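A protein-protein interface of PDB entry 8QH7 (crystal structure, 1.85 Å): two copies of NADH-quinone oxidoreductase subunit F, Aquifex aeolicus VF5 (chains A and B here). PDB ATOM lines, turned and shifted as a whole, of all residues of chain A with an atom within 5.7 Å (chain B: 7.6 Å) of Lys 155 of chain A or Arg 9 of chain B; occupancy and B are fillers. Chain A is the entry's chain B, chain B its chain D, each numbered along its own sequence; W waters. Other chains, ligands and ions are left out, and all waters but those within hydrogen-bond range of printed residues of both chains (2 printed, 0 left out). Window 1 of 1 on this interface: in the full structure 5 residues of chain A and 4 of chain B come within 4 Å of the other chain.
Hydrophobic or aromatic side chains of chain A that line the printed part of chain B: Phe 157 and Leu 163.
Along chain A the printed residues that touch a printed residue of chain B span positions 154 to 163.
Of the 14 printed residues of chain B, 3 touch a printed residue of chain A.
Hydrophobic or aromatic side chains of chain B within 4 Å of the printed part of chain A: Tyr 11 and Pro 26.
Among the printed residues, 6 pairs touch across the chains.
Among the printed residues, no Asp or Glu carboxylate lies within 4 Å of a Lys or Arg side-chain nitrogen of the other chain.
The backbone NH (N) of Phe 157 of chain A sits at hydrogen-bond distance from the backbone carbonyl oxygen (O) of Ala 152 of chain A, 2.9 Å away.
The guanidinium group of Arg 9 of chain B is in hydrogen-bond range of the backbone carbonyl oxygen of Ile 7 of chain B (3.3 Å).
Lys 155 of chain A touches just one residue of chain B: Arg 9 (2.9 Å).
Arg 9 of chain B touches just these residues of chain A: Lys 154 (3.7 Å), Lys 155 (2.9 Å), Phe 157 (3.96 Å) and Leu 163 (3.7 Å).
Printed residues of chain B within 4 Å of Phe 157 of chain A: Arg 9.
Of the printed residues of chain A, Pro 26 of chain B touches Lys 154.
Of the printed residues of chain B, Lys 154 of chain A touches Arg 9 (3.7 Å), Tyr 11 (3.9 Å) and Pro 26 (3.9 Å).
Printed residues of chain B within 4 Å of Leu 163 of chain A: Arg 9 (3.7 Å).
Arg 27 of chain B touches none of the printed residues of chain A.
Lys 25 of chain B touches none of the printed residues of chain A.
The nearest residue of chain B that does not touch Lys 155 of chain A is Pro 26 of chain B (5.1 Å).
No position is printed for both chains.
Of the 6 pairs that touch across the chains among the printed residues, none has its exchanged pair printed and touching as well.
O of Lys 155 of chain A is in hydrogen-bond range of NE of Arg 9 of chain B.
Water W2 bridges O of Lys 154 of chain A (2.6 Å) and O of Ile 10 of chain B (2.8 Å).
Water W1 lies within hydrogen-bond range of the side-chain amino group (NZ) of Lys 155 of chain A (2.8 Å) and the backbone carbonyl oxygen (O) of Arg 9 of chain B (2.9 Å).
Among the printed residues, merely in contact across the chains: Lys 154 of chain A with Arg 9 of chain B (3.7 Å), Lys 154 of chain A with Tyr 11 of chain B (3.9 Å), Lys 154 of chain A with Pro 26 of chain B (3.9 Å), Phe 157 of chain A with Arg 9 of chain B (3.96 Å) and Leu 163 of chain A with Arg 9 of chain B (3.7 Å).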
ATOM      1  N   ILE A  31      23.808  18.668  -2.874  1.00  0.00           N
ATOM      2  CA  ILE A  31      24.606  18.256  -4.015  1.00  0.00           C
ATOM      3  C   ILE A  31      25.404  19.441  -4.566  1.00  0.00           C
ATOM      4  O   ILE A  31      26.536  19.249  -4.984  1.00  0.00           O
ATOM      5  CB  ILE A  31      23.743  17.560  -5.093  1.00  0.00           C
ATOM      6  CG1 ILE A  31      24.601  16.685  -6.010  1.00  0.00           C
ATOM      7  CG2 ILE A  31      22.922  18.567  -5.888  1.00  0.00           C
ATOM      8  CD1 ILE A  31      23.820  15.631  -6.759  1.00  0.00           C
ATOM      9  N   ASP A  32      24.848  20.662  -4.556  1.00  0.00           N
ATOM     10  CA  ASP A  32      25.566  21.810  -5.109  1.00  0.00           C
ATOM     11  C   ASP A  32      26.872  22.064  -4.349  1.00  0.00           C
ATOM     12  O   ASP A  32      27.916  22.296  -4.967  1.00  0.00           O
ATOM     13  CB  ASP A  32      24.703  23.081  -5.137  1.00  0.00           C
ATOM     14  CG  ASP A  32      23.699  23.105  -6.275  1.00  0.00           C
ATOM     15  OD1 ASP A  32      23.682  22.155  -7.079  1.00  0.00           O
ATOM     16  OD2 ASP A  32      22.962  24.083  -6.368  1.00  0.00           O
ATOM     17  N   LEU A  35      29.251  19.344  -5.263  1.00  0.00           N
ATOM     18  CA  LEU A  35      29.793  19.570  -6.598  1.00  0.00           C
ATOM     19  C   LEU A  35      30.845  20.688  -6.605  1.00  0.00           C
ATOM     20  O   LEU A  35      31.837  20.610  -7.335  1.00  0.00           O
ATOM     21  CB  LEU A  35      28.625  19.887  -7.537  1.00  0.00           C
ATOM     22  CG  LEU A  35      27.722  18.692  -7.847  1.00  0.00           C
ATOM     23  CD1 LEU A  35      26.442  19.125  -8.540  1.00  0.00           C
ATOM     24  CD2 LEU A  35      28.462  17.685  -8.709  1.00  0.00           C
ATOM     25  N   GLU A  44      32.897  10.147 -12.508  1.00  0.00           N
ATOM     26  CA  GLU A  44      33.102  10.347 -13.937  1.00  0.00           C
ATOM     27  C   GLU A  44      34.391   9.666 -14.391  1.00  0.00           C
ATOM     28  O   GLU A  44      34.424   9.039 -15.442  1.00  0.00           O
ATOM     29  CB  GLU A  44      33.191  11.832 -14.269  1.00  0.00           C
ATOM     30  CG  GLU A  44      31.959  12.622 -13.881  1.00  0.00           C
ATOM     31  CD  GLU A  44      32.092  14.089 -14.247  1.00  0.00           C
ATOM     32  OE1 GLU A  44      31.994  14.398 -15.450  1.00  0.00           O
ATOM     33  OE2 GLU A  44      32.350  14.905 -13.334  1.00  0.00           O
ATOM     34  N   GLU A 150      17.532  11.546  -4.696  1.00  0.00           N
ATOM     35  CA  GLU A 150      16.766  12.267  -5.702  1.00  0.00           C
ATOM     36  C   GLU A 150      17.599  13.379  -6.348  1.00  0.00           C
ATOM     37  O   GLU A 150      17.451  13.634  -7.549  1.00  0.00           O
ATOM     38  CB  GLU A 150      15.479  12.842  -5.105  1.00  0.00           C
ATOM     39  CG  GLU A 150      14.461  11.794  -4.708  1.00  0.00           C
ATOM     40  CD  GLU A 150      14.032  10.859  -5.828  1.00  0.00           C
ATOM     41  OE1 GLU A 150      13.721  11.362  -6.924  1.00  0.00           O
ATOM     42  OE2 GLU A 150      14.032   9.629  -5.594  1.00  0.00           O
ATOM     43  N   GLU A 151      18.444  14.064  -5.561  1.00  0.00           N
ATOM     44  CA  GLU A 151      19.358  15.058  -6.118  1.00  0.00           C
ATOM     45  C   GLU A 151      20.310  14.415  -7.130  1.00  0.00           C
ATOM     46  O   GLU A 151      20.559  14.985  -8.192  1.00  0.00           O
ATOM     47  CB  GLU A 151      20.226  15.726  -5.052  1.00  0.00           C
ATOM     48  CG  GLU A 151      19.478  16.624  -4.087  1.00  0.00           C
ATOM     49  CD  GLU A 151      20.409  17.237  -3.049  1.00  0.00           C
ATOM     50  OE1 GLU A 151      20.543  18.473  -3.044  1.00  0.00           O
ATOM     51  OE2 GLU A 151      21.040  16.481  -2.285  1.00  0.00           O
ATOM     52  N   ALA A 152      20.845  13.235  -6.785  1.00  0.00           N
ATOM     53  CA  ALA A 152      21.758  12.507  -7.653  1.00  0.00           C
ATOM     54  C   ALA A 152      21.059  12.104  -8.958  1.00  0.00           C
ATOM     55  O   ALA A 152      21.664  12.187 -10.029  1.00  0.00           O
ATOM     56  CB  ALA A 152      22.326  11.313  -6.926  1.00  0.00           C
ATOM     57  N   LYS A 153      19.787  11.693  -8.863  1.00  0.00           N
ATOM     58  CA  LYS A 153      18.994  11.357 -10.041  1.00  0.00           C
ATOM     59  C   LYS A 153      18.830  12.583 -10.941  1.00  0.00           C
ATOM     60  O   LYS A 153      19.028  12.488 -12.152  1.00  0.00           O
ATOM     61  CB  LYS A 153      17.626  10.795  -9.635  1.00  0.00           C
ATOM     62  CG  LYS A 153      17.659   9.394  -9.042  1.00  0.00           C
ATOM     63  CD  LYS A 153      16.291   8.802  -8.737  1.00  0.00           C
ATOM     64  CE  LYS A 153      15.424   8.627  -9.966  1.00  0.00           C
ATOM     65  NZ  LYS A 153      14.508   7.465  -9.836  1.00  0.00           N
ATOM     66  N   LYS A 154      18.472  13.729 -10.342  1.00  0.00           N
ATOM     67  CA  LYS A 154      18.310  14.989 -11.068  1.00  0.00           C
ATOM     68  C   LYS A 154      19.557  15.326 -11.893  1.00  0.00           C
ATOM     69  O   LYS A 154      19.437  15.845 -13.002  1.00  0.00           O
ATOM     70  CB  LYS A 154      18.010  16.159 -10.113  1.00  0.00           C
ATOM     71  CG  LYS A 154      18.450  17.546 -10.597  1.00  0.00           C
ATOM     72  CD  LYS A 154      18.452  18.664  -9.546  1.00  0.00           C
ATOM     73  CE  LYS A 154      19.175  18.275  -8.268  1.00  0.00           C
ATOM     74  NZ  LYS A 154      19.363  19.442  -7.370  1.00  0.00           N
ATOM     75  N   LYS A 155      20.743  15.050 -11.334  1.00  0.00           N
ATOM     76  CA  LYS A 155      22.006  15.430 -11.945  1.00  0.00           C
ATOM     77  C   LYS A 155      22.565  14.317 -12.826  1.00  0.00           C
ATOM     78  O   LYS A 155      23.663  14.465 -13.356  1.00  0.00           O
ATOM     79  CB  LYS A 155      23.033  15.804 -10.870  1.00  0.00           C
ATOM     80  CG  LYS A 155      22.752  17.103 -10.132  1.00  0.00           C
ATOM     81  CD  LYS A 155      22.779  18.318 -11.040  1.00  0.00           C
ATOM     82  CE  LYS A 155      22.956  19.613 -10.277  1.00  0.00           C
ATOM     83  NZ  LYS A 155      22.857  20.790 -11.172  1.00  0.00           N
ATOM     84  N   GLY A 156      21.838  13.197 -12.942  1.00  0.00           N
ATOM     85  CA  GLY A 156      22.178  12.132 -13.875  1.00  0.00           C
ATOM     86  C   GLY A 156      23.278  11.188 -13.382  1.00  0.00           C
ATOM     87  O   GLY A 156      23.935  10.533 -14.181  1.00  0.00           O
ATOM     88  N   PHE A 157      23.450  11.079 -12.057  1.00  0.00           N
ATOM     89  CA  PHE A 157      24.446  10.191 -11.480  1.00  0.00           C
ATOM     90  C   PHE A 157      23.827   8.839 -11.127  1.00  0.00           C
ATOM     91  O   PHE A 157      24.558   7.907 -10.801  1.00  0.00           O
ATOM     92  CB  PHE A 157      25.083  10.840 -10.250  1.00  0.00           C
ATOM     93  CG  PHE A 157      25.802  12.131 -10.548  1.00  0.00           C
ATOM     94  CD1 PHE A 157      26.748  12.200 -11.559  1.00  0.00           C
ATOM     95  CD2 PHE A 157      25.520  13.284  -9.829  1.00  0.00           C
ATOM     96  CE1 PHE A 157      27.397  13.394 -11.847  1.00  0.00           C
ATOM     97  CE2 PHE A 157      26.189  14.469 -10.098  1.00  0.00           C
ATOM     98  CZ  PHE A 157      27.117  14.529 -11.116  1.00  0.00           C
ATOM     99  N   LEU A 163      25.586   8.923 -17.447  1.00  0.00           N
ATOM    100  CA  LEU A 163      26.561   9.767 -18.128  1.00  0.00           C
ATOM    101  C   LEU A 163      27.048   9.109 -19.420  1.00  0.00           C
ATOM    102  O   LEU A 163      28.212   9.252 -19.788  1.00  0.00           O
ATOM    103  CB  LEU A 163      27.723  10.057 -17.173  1.00  0.00           C
ATOM    104  CG  LEU A 163      27.337  10.747 -15.862  1.00  0.00           C
ATOM    105  CD1 LEU A 163      28.555  10.970 -14.975  1.00  0.00           C
ATOM    106  CD2 LEU A 163      26.618  12.063 -16.132  1.00  0.00           C
ATOM    107  N   ALA B   6      28.892  15.991 -23.976  1.00  0.00           N
ATOM    108  CA  ALA B   6      28.328  16.246 -22.659  1.00  0.00           C
ATOM    109  C   ALA B   6      27.278  17.355 -22.722  1.00  0.00           C
ATOM    110  O   ALA B   6      27.458  18.379 -23.389  1.00  0.00           O
ATOM    111  CB  ALA B   6      29.427  16.583 -21.680  1.00  0.00           C
ATOM    112  N   ILE B   7      26.169  17.114 -22.011  1.00  0.00           N
ATOM    113  CA  ILE B   7      25.076  18.059 -21.848  1.00  0.00           C
ATOM    114  C   ILE B   7      24.839  18.222 -20.352  1.00  0.00           C
ATOM    115  O   ILE B   7      24.645  17.215 -19.683  1.00  0.00           O
ATOM    116  CB  ILE B   7      23.776  17.512 -22.461  1.00  0.00           C
ATOM    117  CG1 ILE B   7      23.928  17.070 -23.920  1.00  0.00           C
ATOM    118  CG2 ILE B   7      22.653  18.520 -22.269  1.00  0.00           C
ATOM    119  CD1 ILE B   7      22.808  16.151 -24.370  1.00  0.00           C
ATOM    120  N   PRO B   8      24.776  19.446 -19.782  1.00  0.00           N
ATOM    121  CA  PRO B   8      24.430  19.583 -18.369  1.00  0.00           C
ATOM    122  C   PRO B   8      23.007  19.072 -18.152  1.00  0.00           C
ATOM    123  O   PRO B   8      22.175  19.108 -19.066  1.00  0.00           O
ATOM    124  CB  PRO B   8      24.619  21.085 -18.086  1.00  0.00           C
ATOM    125  CG  PRO B   8      24.483  21.760 -19.441  1.00  0.00           C
ATOM    126  CD  PRO B   8      24.968  20.744 -20.456  1.00  0.00           C
ATOM    127  N   ARG B   9      22.760  18.532 -16.953  1.00  0.00           N
ATOM    128  CA  ARG B   9      21.516  17.847 -16.646  1.00  0.00           C
ATOM    129  C   ARG B   9      20.526  18.851 -16.062  1.00  0.00           C
ATOM    130  O   ARG B   9      20.503  19.109 -14.842  1.00  0.00           O
ATOM    131  CB  ARG B   9      21.772  16.668 -15.698  1.00  0.00           C
ATOM    132  CG  ARG B   9      22.207  15.387 -16.398  1.00  0.00           C
ATOM    133  CD  ARG B   9      23.620  15.440 -16.944  1.00  0.00           C
ATOM    134  NE  ARG B   9      24.589  15.525 -15.862  1.00  0.00           N
ATOM    135  CZ  ARG B   9      25.893  15.699 -16.029  1.00  0.00           C
ATOM    136  NH1 ARG B   9      26.689  15.716 -14.975  1.00  0.00           N
ATOM    137  NH2 ARG B   9      26.387  15.861 -17.248  1.00  0.00           N
ATOM    138  N   ILE B  10      19.768  19.471 -16.971  1.00  0.00           N
ATOM    139  CA  ILE B  10      18.764  20.461 -16.617  1.00  0.00           C
ATOM    140  C   ILE B  10      17.651  19.732 -15.863  1.00  0.00           C
ATOM    141  O   ILE B  10      17.212  18.665 -16.292  1.00  0.00           O
ATOM    142  CB  ILE B  10      18.260  21.181 -17.889  1.00  0.00           C
ATOM    143  CG1 ILE B  10      19.372  22.016 -18.536  1.00  0.00           C
ATOM    144  CG2 ILE B  10      17.011  22.010 -17.603  1.00  0.00           C
ATOM    145  CD1 ILE B  10      19.119  22.389 -19.981  1.00  0.00           C
ATOM    146  N   TYR B  11      17.233  20.302 -14.724  1.00  0.00           N
ATOM    147  CA  TYR B  11      16.120  19.762 -13.963  1.00  0.00           C
ATOM    148  C   TYR B  11      14.825  19.960 -14.753  1.00  0.00           C
ATOM    149  O   TYR B  11      14.618  21.018 -15.343  1.00  0.00           O
ATOM    150  CB  TYR B  11      16.018  20.436 -12.593  1.00  0.00           C
ATOM    151  CG  TYR B  11      14.838  19.959 -11.783  1.00  0.00           C
ATOM    152  CD1 TYR B  11      14.750  18.636 -11.373  1.00  0.00           C
ATOM    153  CD2 TYR B  11      13.782  20.805 -11.479  1.00  0.00           C
ATOM    154  CE1 TYR B  11      13.662  18.170 -10.648  1.00  0.00           C
ATOM    155  CE2 TYR B  11      12.678  20.355 -10.772  1.00  0.00           C
ATOM    156  CZ  TYR B  11      12.629  19.037 -10.332  1.00  0.00           C
ATOM    157  OH  TYR B  11      11.555  18.562  -9.617  1.00  0.00           O
ATOM    158  N   ALA B  12      13.948  18.948 -14.736  1.00  0.00           N
ATOM    159  CA  ALA B  12      12.655  19.039 -15.399  1.00  0.00           C
ATOM    160  C   ALA B  12      11.567  18.386 -14.538  1.00  0.00           C
ATOM    161  O   ALA B  12      11.790  17.345 -13.912  1.00  0.00           O
ATOM    162  CB  ALA B  12      12.748  18.422 -16.773  1.00  0.00           C
ATOM    163  N   LYS B  25      13.422  12.731 -17.379  1.00  0.00           N
ATOM    164  CA  LYS B  25      14.640  12.008 -17.055  1.00  0.00           C
ATOM    165  C   LYS B  25      15.732  12.454 -18.022  1.00  0.00           C
ATOM    166  O   LYS B  25      15.523  12.459 -19.247  1.00  0.00           O
ATOM    167  CB  LYS B  25      14.415  10.492 -17.100  1.00  0.00           C
ATOM    168  CG  LYS B  25      13.284   9.974 -16.218  1.00  0.00           C
ATOM    169  CD  LYS B  25      13.475  10.260 -14.744  1.00  0.00           C
ATOM    170  N   PRO B  26      16.913  12.869 -17.500  1.00  0.00           N
ATOM    171  CA  PRO B  26      17.938  13.517 -18.319  1.00  0.00           C
ATOM    172  C   PRO B  26      18.842  12.543 -19.065  1.00  0.00           C
ATOM    173  O   PRO B  26      20.000  12.338 -18.706  1.00  0.00           O
ATOM    174  CB  PRO B  26      18.711  14.330 -17.271  1.00  0.00           C
ATOM    175  CG  PRO B  26      18.662  13.472 -16.032  1.00  0.00           C
ATOM    176  CD  PRO B  26      17.300  12.802 -16.075  1.00  0.00           C
ATOM    177  N   ARG B  27      18.283  11.919 -20.103  1.00  0.00           N
ATOM    178  CA  ARG B  27      19.031  10.979 -20.915  1.00  0.00           C
ATOM    179  C   ARG B  27      18.275  10.802 -22.227  1.00  0.00           C
ATOM    180  O   ARG B  27      17.096  11.130 -22.299  1.00  0.00           O
ATOM    181  CB  ARG B  27      19.221   9.630 -20.203  1.00  0.00           C
ATOM    182  CG  ARG B  27      17.941   8.830 -19.991  1.00  0.00           C
ATOM    183  CD  ARG B  27      18.151   7.496 -19.287  1.00  0.00           C
ATOM    184  NE  ARG B  27      16.907   6.796 -18.963  1.00  0.00           N
ATOM    185  CZ  ARG B  27      16.150   6.129 -19.837  1.00  0.00           C
ATOM    186  NH1 ARG B  27      15.059   5.501 -19.433  1.00  0.00           N
ATOM    187  NH2 ARG B  27      16.476   6.097 -21.118  1.00  0.00           N
ATOM    188  N   ILE B 105      15.413  20.151 -24.322  1.00  0.00           N
ATOM    189  CA  ILE B 105      15.217  18.961 -23.502  1.00  0.00           C
ATOM    190  C   ILE B 105      14.367  17.929 -24.264  1.00  0.00           C
ATOM    191  O   ILE B 105      14.586  16.726 -24.097  1.00  0.00           O
ATOM    192  CB  ILE B 105      14.693  19.243 -22.080  1.00  0.00           C
ATOM    193  CG1 ILE B 105      13.274  19.801 -22.074  1.00  0.00           C
ATOM    194  CG2 ILE B 105      15.655  20.114 -21.271  1.00  0.00           C
ATOM    195  CD1 ILE B 105      12.654  19.776 -20.717  1.00  0.00           C
ATOM    196  N   ARG B 109      16.367  14.441 -25.198  1.00  0.00           N
ATOM    197  CA  ARG B 109      15.913  13.378 -24.304  1.00  0.00           C
ATOM    198  C   ARG B 109      14.783  12.543 -24.906  1.00  0.00           C
ATOM    199  O   ARG B 109      14.668  11.368 -24.568  1.00  0.00           O
ATOM    200  CB  ARG B 109      15.440  13.939 -22.965  1.00  0.00           C
ATOM    201  CG  ARG B 109      16.526  14.697 -22.221  1.00  0.00           C
ATOM    202  CD  ARG B 109      15.974  15.395 -21.001  1.00  0.00           C
ATOM    203  NE  ARG B 109      17.017  16.182 -20.368  1.00  0.00           N
ATOM    204  CZ  ARG B 109      16.890  16.760 -19.183  1.00  0.00           C
ATOM    205  NH1 ARG B 109      17.889  17.458 -18.675  1.00  0.00           N
ATOM    206  NH2 ARG B 109      15.768  16.590 -18.500  1.00  0.00           N
ATOM    207  N   PRO B 261      16.013  25.949 -10.561  1.00  0.00           N
ATOM    208  CA  PRO B 261      16.006  26.337 -11.971  1.00  0.00           C
ATOM    209  C   PRO B 261      15.894  25.086 -12.836  1.00  0.00           C
ATOM    210  O   PRO B 261      16.432  24.026 -12.481  1.00  0.00           O
ATOM    211  CB  PRO B 261      17.333  27.084 -12.161  1.00  0.00           C
ATOM    212  CG  PRO B 261      18.231  26.515 -11.082  1.00  0.00           C
ATOM    213  CD  PRO B 261      17.314  26.192  -9.920  1.00  0.00           C
ATOM    214  N   GLY B 262      15.126  25.210 -13.922  1.00  0.00           N
ATOM    215  CA  GLY B 262      14.775  24.063 -14.740  1.00  0.00           C
ATOM    216  C   GLY B 262      13.569  24.326 -15.635  1.00  0.00           C
ATOM    217  O   GLY B 262      13.092  25.458 -15.749  1.00  0.00           O
HETATM  218  O   HOH W   1      20.270  20.455 -12.263  1.00  0.00           O
HETATM  219  O   HOH W   2      17.496  16.356 -14.722  1.00  0.00           O
